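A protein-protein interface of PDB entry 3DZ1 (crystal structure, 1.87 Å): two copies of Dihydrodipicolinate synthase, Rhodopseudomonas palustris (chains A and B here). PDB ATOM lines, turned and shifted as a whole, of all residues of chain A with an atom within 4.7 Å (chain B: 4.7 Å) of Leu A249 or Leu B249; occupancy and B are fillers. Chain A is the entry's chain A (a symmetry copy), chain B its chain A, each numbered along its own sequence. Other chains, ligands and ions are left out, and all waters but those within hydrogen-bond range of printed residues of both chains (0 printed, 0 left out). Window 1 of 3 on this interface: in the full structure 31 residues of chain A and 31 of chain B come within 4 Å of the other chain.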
ATOM      1  N   LEU A 203      23.987  -1.673   9.332  1.00  0.00           N
ATOM      2  CA  LEU A 203      23.309  -2.839   9.878  1.00  0.00           C
ATOM      3  C   LEU A 203      23.886  -4.173   9.405  1.00  0.00           C
ATOM      4  O   LEU A 203      23.852  -5.154  10.143  1.00  0.00           O
ATOM      5  CB  LEU A 203      21.813  -2.762   9.550  1.00  0.00           C
ATOM      6  CG  LEU A 203      20.841  -3.597  10.389  1.00  0.00           C
ATOM      7  CD1 LEU A 203      20.843  -3.102  11.825  1.00  0.00           C
ATOM      8  CD2 LEU A 203      19.439  -3.481   9.796  1.00  0.00           C
ATOM      9  N   PHE A 245      32.166  -5.729  15.636  1.00  0.00           N
ATOM     10  CA  PHE A 245      30.897  -5.316  15.058  1.00  0.00           C
ATOM     11  C   PHE A 245      29.766  -5.626  16.042  1.00  0.00           C
ATOM     12  O   PHE A 245      28.946  -4.763  16.351  1.00  0.00           O
ATOM     13  CB  PHE A 245      30.647  -6.045  13.728  1.00  0.00           C
ATOM     14  CG  PHE A 245      29.357  -5.661  13.065  1.00  0.00           C
ATOM     15  CD1 PHE A 245      29.251  -4.471  12.347  1.00  0.00           C
ATOM     16  CD2 PHE A 245      28.234  -6.474  13.184  1.00  0.00           C
ATOM     17  CE1 PHE A 245      28.042  -4.098  11.756  1.00  0.00           C
ATOM     18  CE2 PHE A 245      27.021  -6.111  12.599  1.00  0.00           C
ATOM     19  CZ  PHE A 245      26.927  -4.920  11.883  1.00  0.00           C
ATOM     20  N   ASP A 246      29.739  -6.858  16.543  1.00  0.00           N
ATOM     21  CA  ASP A 246      28.700  -7.289  17.481  1.00  0.00           C
ATOM     22  C   ASP A 246      28.618  -6.439  18.739  1.00  0.00           C
ATOM     23  O   ASP A 246      27.539  -6.296  19.332  1.00  0.00           O
ATOM     24  CB  ASP A 246      28.914  -8.751  17.884  1.00  0.00           C
ATOM     25  CG  ASP A 246      28.604  -9.715  16.760  1.00  0.00           C
ATOM     26  OD1 ASP A 246      28.162  -9.260  15.680  1.00  0.00           O
ATOM     27  OD2 ASP A 246      28.795 -10.931  16.960  1.00  0.00           O
ATOM     28  N   ALA A 247      29.757  -5.899  19.162  1.00  0.00           N
ATOM     29  CA  ALA A 247      29.800  -5.056  20.345  1.00  0.00           C
ATOM     30  C   ALA A 247      29.104  -3.735  20.038  1.00  0.00           C
ATOM     31  O   ALA A 247      28.515  -3.110  20.917  1.00  0.00           O
ATOM     32  CB  ALA A 247      31.251  -4.812  20.769  1.00  0.00           C
ATOM     33  N   HIS A 248      29.162  -3.320  18.778  1.00  0.00           N
ATOM     34  CA  HIS A 248      28.530  -2.073  18.365  1.00  0.00           C
ATOM     35  C   HIS A 248      27.113  -2.235  17.832  1.00  0.00           C
ATOM     36  O   HIS A 248      26.357  -1.274  17.782  1.00  0.00           O
ATOM     37  CB  HIS A 248      29.397  -1.383  17.308  1.00  0.00           C
ATOM     38  CG  HIS A 248      30.582  -0.677  17.885  1.00  0.00           C
ATOM     39  ND1 HIS A 248      30.544   0.649  18.261  1.00  0.00           N
ATOM     40  CD2 HIS A 248      31.806  -1.134  18.237  1.00  0.00           C
ATOM     41  CE1 HIS A 248      31.693   0.977  18.823  1.00  0.00           C
ATOM     42  NE2 HIS A 248      32.476  -0.087  18.822  1.00  0.00           N
ATOM     43  N   LEU A 249      26.742  -3.450  17.452  1.00  0.00           N
ATOM     44  CA  LEU A 249      25.416  -3.673  16.884  1.00  0.00           C
ATOM     45  C   LEU A 249      24.244  -3.136  17.708  1.00  0.00           C
ATOM     46  O   LEU A 249      23.287  -2.600  17.145  1.00  0.00           O
ATOM     47  CB  LEU A 249      25.216  -5.162  16.586  1.00  0.00           C
ATOM     48  CG  LEU A 249      23.955  -5.499  15.787  1.00  0.00           C
ATOM     49  CD1 LEU A 249      23.928  -4.691  14.490  1.00  0.00           C
ATOM     50  CD2 LEU A 249      23.929  -6.994  15.491  1.00  0.00           C
ATOM     51  N   PRO A 250      24.292  -3.272  19.043  1.00  0.00           N
ATOM     52  CA  PRO A 250      23.172  -2.754  19.837  1.00  0.00           C
ATOM     53  C   PRO A 250      22.949  -1.260  19.602  1.00  0.00           C
ATOM     54  O   PRO A 250      21.813  -0.814  19.457  1.00  0.00           O
ATOM     55  CB  PRO A 250      23.597  -3.063  21.270  1.00  0.00           C
ATOM     56  CG  PRO A 250      24.336  -4.353  21.107  1.00  0.00           C
ATOM     57  CD  PRO A 250      25.206  -4.062  19.887  1.00  0.00           C
ATOM     58  N   LEU A 251      24.034  -0.489  19.555  1.00  0.00           N
ATOM     59  CA  LEU A 251      23.929   0.952  19.332  1.00  0.00           C
ATOM     60  C   LEU A 251      23.695   1.249  17.861  1.00  0.00           C
ATOM     61  O   LEU A 251      22.976   2.182  17.517  1.00  0.00           O
ATOM     62  CB  LEU A 251      25.190   1.669  19.822  1.00  0.00           C
ATOM     63  CG  LEU A 251      25.194   3.194  19.684  1.00  0.00           C
ATOM     64  CD1 LEU A 251      24.017   3.788  20.447  1.00  0.00           C
ATOM     65  CD2 LEU A 251      26.519   3.746  20.209  1.00  0.00           C
ATOM     66  N   ILE A 252      24.308   0.463  16.984  1.00  0.00           N
ATOM     67  CA  ILE A 252      24.107   0.652  15.555  1.00  0.00           C
ATOM     68  C   ILE A 252      22.613   0.530  15.252  1.00  0.00           C
ATOM     69  O   ILE A 252      22.043   1.359  14.538  1.00  0.00           O
ATOM     70  CB  ILE A 252      24.875  -0.416  14.734  1.00  0.00           C
ATOM     71  CG1 ILE A 252      26.373  -0.106  14.767  1.00  0.00           C
ATOM     72  CG2 ILE A 252      24.339  -0.469  13.300  1.00  0.00           C
ATOM     73  CD1 ILE A 252      27.249  -1.184  14.147  1.00  0.00           C
ATOM     74  N   ARG A 253      21.969  -0.497  15.800  1.00  0.00           N
ATOM     75  CA  ARG A 253      20.547  -0.677  15.534  1.00  0.00           C
ATOM     76  C   ARG A 253      19.671   0.368  16.214  1.00  0.00           C
ATOM     77  O   ARG A 253      18.620   0.726  15.685  1.00  0.00           O
ATOM     78  CB  ARG A 253      20.088  -2.097  15.908  1.00  0.00           C
ATOM     79  CG  ARG A 253      20.190  -2.451  17.359  1.00  0.00           C
ATOM     80  CD  ARG A 253      18.965  -2.009  18.158  1.00  0.00           C
ATOM     81  NE  ARG A 253      19.343  -1.887  19.555  1.00  0.00           N
ATOM     82  CZ  ARG A 253      18.716  -2.462  20.574  1.00  0.00           C
ATOM     83  NH1 ARG A 253      17.647  -3.217  20.371  1.00  0.00           N
ATOM     84  NH2 ARG A 253      19.184  -2.288  21.801  1.00  0.00           N
ATOM     85  N   LEU B 203      13.677  -6.708  17.119  1.00  0.00           N
ATOM     86  CA  LEU B 203      14.795  -5.784  16.998  1.00  0.00           C
ATOM     87  C   LEU B 203      14.979  -4.868  18.209  1.00  0.00           C
ATOM     88  O   LEU B 203      16.102  -4.486  18.526  1.00  0.00           O
ATOM     89  CB  LEU B 203      14.634  -4.949  15.722  1.00  0.00           C
ATOM     90  CG  LEU B 203      15.873  -4.261  15.142  1.00  0.00           C
ATOM     91  CD1 LEU B 203      16.871  -5.307  14.675  1.00  0.00           C
ATOM     92  CD2 LEU B 203      15.454  -3.376  13.972  1.00  0.00           C
ATOM     93  N   PHE B 245      20.242 -10.762  25.091  1.00  0.00           N
ATOM     94  CA  PHE B 245      19.674 -10.166  23.892  1.00  0.00           C
ATOM     95  C   PHE B 245      20.799  -9.852  22.901  1.00  0.00           C
ATOM     96  O   PHE B 245      20.731 -10.227  21.731  1.00  0.00           O
ATOM     97  CB  PHE B 245      18.911  -8.879  24.239  1.00  0.00           C
ATOM     98  CG  PHE B 245      18.287  -8.210  23.050  1.00  0.00           C
ATOM     99  CD1 PHE B 245      17.093  -8.685  22.509  1.00  0.00           C
ATOM    100  CD2 PHE B 245      18.909  -7.121  22.446  1.00  0.00           C
ATOM    101  CE1 PHE B 245      16.529  -8.082  21.383  1.00  0.00           C
ATOM    102  CE2 PHE B 245      18.355  -6.513  21.320  1.00  0.00           C
ATOM    103  CZ  PHE B 245      17.161  -6.995  20.789  1.00  0.00           C
ATOM    104  N   ASP B 246      21.840  -9.178  23.382  1.00  0.00           N
ATOM    105  CA  ASP B 246      22.974  -8.799  22.536  1.00  0.00           C
ATOM    106  C   ASP B 246      23.653  -9.978  21.856  1.00  0.00           C
ATOM    107  O   ASP B 246      24.211  -9.834  20.759  1.00  0.00           O
ATOM    108  CB  ASP B 246      24.017  -8.029  23.351  1.00  0.00           C
ATOM    109  CG  ASP B 246      23.553  -6.638  23.724  1.00  0.00           C
ATOM    110  OD1 ASP B 246      22.443  -6.240  23.302  1.00  0.00           O
ATOM    111  OD2 ASP B 246      24.303  -5.940  24.435  1.00  0.00           O
ATOM    112  N   ALA B 247      23.632 -11.132  22.515  1.00  0.00           N
ATOM    113  CA  ALA B 247      24.235 -12.331  21.959  1.00  0.00           C
ATOM    114  C   ALA B 247      23.396 -12.807  20.779  1.00  0.00           C
ATOM    115  O   ALA B 247      23.912 -13.392  19.829  1.00  0.00           O
ATOM    116  CB  ALA B 247      24.326 -13.424  23.028  1.00  0.00           C
ATOM    117  N   HIS B 248      22.097 -12.539  20.836  1.00  0.00           N
ATOM    118  CA  HIS B 248      21.195 -12.943  19.765  1.00  0.00           C
ATOM    119  C   HIS B 248      20.966 -11.875  18.704  1.00  0.00           C
ATOM    120  O   HIS B 248      20.532 -12.182  17.601  1.00  0.00           O
ATOM    121  CB  HIS B 248      19.850 -13.369  20.358  1.00  0.00           C
ATOM    122  CG  HIS B 248      19.874 -14.741  20.953  1.00  0.00           C
ATOM    123  ND1 HIS B 248      19.552 -15.869  20.228  1.00  0.00           N
ATOM    124  CD2 HIS B 248      20.272 -15.176  22.171  1.00  0.00           C
ATOM    125  CE1 HIS B 248      19.754 -16.940  20.974  1.00  0.00           C
ATOM    126  NE2 HIS B 248      20.192 -16.548  22.157  1.00  0.00           N
ATOM    127  N   LEU B 249      21.274 -10.626  19.023  1.00  0.00           N
ATOM    128  CA  LEU B 249      21.034  -9.542  18.075  1.00  0.00           C
ATOM    129  C   LEU B 249      21.608  -9.750  16.672  1.00  0.00           C
ATOM    130  O   LEU B 249      20.962  -9.403  15.682  1.00  0.00           O
ATOM    131  CB  LEU B 249      21.530  -8.215  18.659  1.00  0.00           C
ATOM    132  CG  LEU B 249      21.139  -6.970  17.859  1.00  0.00           C
ATOM    133  CD1 LEU B 249      19.625  -6.930  17.663  1.00  0.00           C
ATOM    134  CD2 LEU B 249      21.620  -5.725  18.595  1.00  0.00           C
ATOM    135  N   PRO B 250      22.825 -10.309  16.560  1.00  0.00           N
ATOM    136  CA  PRO B 250      23.376 -10.514  15.217  1.00  0.00           C
ATOM    137  C   PRO B 250      22.463 -11.384  14.352  1.00  0.00           C
ATOM    138  O   PRO B 250      22.241 -11.082  13.182  1.00  0.00           O
ATOM    139  CB  PRO B 250      24.721 -11.179  15.498  1.00  0.00           C
ATOM    140  CG  PRO B 250      25.135 -10.523  16.777  1.00  0.00           C
ATOM    141  CD  PRO B 250      23.844 -10.583  17.589  1.00  0.00           C
ATOM    142  N   LEU B 251      21.928 -12.456  14.931  1.00  0.00           N
ATOM    143  CA  LEU B 251      21.039 -13.350  14.192  1.00  0.00           C
ATOM    144  C   LEU B 251      19.647 -12.753  14.087  1.00  0.00           C
ATOM    145  O   LEU B 251      18.968 -12.918  13.078  1.00  0.00           O
ATOM    146  CB  LEU B 251      20.975 -14.727  14.860  1.00  0.00           C
ATOM    147  CG  LEU B 251      20.106 -15.776  14.162  1.00  0.00           C
ATOM    148  CD1 LEU B 251      20.600 -15.994  12.737  1.00  0.00           C
ATOM    149  CD2 LEU B 251      20.147 -17.079  14.959  1.00  0.00           C
ATOM    150  N   ILE B 252      19.208 -12.064  15.134  1.00  0.00           N
ATOM    151  CA  ILE B 252      17.902 -11.423  15.103  1.00  0.00           C
ATOM    152  C   ILE B 252      17.860 -10.456  13.920  1.00  0.00           C
ATOM    153  O   ILE B 252      16.897 -10.441  13.149  1.00  0.00           O
ATOM    154  CB  ILE B 252      17.634 -10.630  16.408  1.00  0.00           C
ATOM    155  CG1 ILE B 252      17.349 -11.608  17.551  1.00  0.00           C
ATOM    156  CG2 ILE B 252      16.478  -9.647  16.204  1.00  0.00           C
ATOM    157  CD1 ILE B 252      17.249 -10.957  18.922  1.00  0.00           C
ATOM    158  N   ARG B 253      18.907  -9.651  13.761  1.00  0.00           N
ATOM    159  CA  ARG B 253      18.918  -8.695  12.661  1.00  0.00           C
ATOM    160  C   ARG B 253      19.087  -9.351  11.297  1.00  0.00           C
ATOM    161  O   ARG B 253      18.566  -8.845  10.304  1.00  0.00           O
ATOM    162  CB  ARG B 253      19.988  -7.611  12.878  1.00  0.00           C
ATOM    163  CG  ARG B 253      21.405  -8.093  12.898  1.00  0.00           C
ATOM    164  CD  ARG B 253      22.010  -8.193  11.499  1.00  0.00           C
ATOM    165  NE  ARG B 253      23.118  -9.132  11.541  1.00  0.00           N
ATOM    166  CZ  ARG B 253      24.348  -8.890  11.106  1.00  0.00           C
ATOM    167  NH1 ARG B 253      24.658  -7.716  10.574  1.00  0.00           N
ATOM    168  NH2 ARG B 253      25.273  -9.830  11.228  1.00  0.00           N
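The backbone carbonyl oxygen (O) of Leu B203 is in hydrogen-bond range of the guanidinium group (NH1) of Arg A253 (2.7 Å).
NH1 of Arg B253 is in hydrogen-bond range of O of Leu A203 (2.7 Å).
NE of Arg B253 lies within hydrogen-bond range of O of Pro B250 (2.7 Å).
The backbone carbonyl oxygen (O) of Pro A250 lies within hydrogen-bond range of the guanidinium group (NE) of Arg A253, at 2.7 Å.
Among the printed residues, merely in contact across the chains: Phe A245 with Arg B253 (3.5 Å), Asp A246 with Pro B250 (3.5 Å), Leu A249 with Leu B249 (3.7 Å), Leu A249 with Pro B250 (3.6 Å), Leu A249 with Arg B253 (3.8 Å), Pro A250 with Asp B246 (3.5 Å), Pro A250 with Leu B249 (3.6 Å), Arg A253 with Phe B245 (3.5 Å) and Arg A253 with Leu B249 (3.8 Å).
Leu A249 touches just these residues of chain B: Leu B249, Pro B250 and Arg B253.
Leu B249 touches just these residues of chain A: Leu A249, Pro A250 and Arg A253.
Of the printed residues of chain A, Phe B245 touches Arg A253.
Of the printed residues of chain A, Arg B253 touches Leu A203, Phe A245 and Leu A249.
Leu A251 touches none of the printed residues of chain B.
The nearest printed residue of chain A that does not touch Leu B249 is Leu A251 (5.8 Å).
The nearest printed residue of chain B that does not touch Arg A253 is Asp B246 (5.3 Å).
Of the 10 printed residues of chain A, 6 touch a printed residue of chain B.
Hydrophobic or aromatic side chains of chain B within 4 Å of the printed part of chain A: Phe B245, Leu B249 and Pro B250.
Along chain B the printed residues that touch a printed residue of chain A span positions 203 to 253.
Among the printed residues, no Asp or Glu carboxylate lies within 4 Å of a Lys or Arg side-chain nitrogen of the other chain.
Leu A203 touches Arg B253, and with the chains exchanged Arg A253 touches Leu B203.
Asp A246 touches Pro B250, and with the chains exchanged Pro A250 touches Asp B246.
Leu B249 touches its own counterpart, Leu A249.
Leu A249 touches Pro B250, and with the chains exchanged Pro A250 touches Leu B249.
Of the 11 pairs that touch across the chains among the printed residues, 11 have their exchanged pair printed and touching as well.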
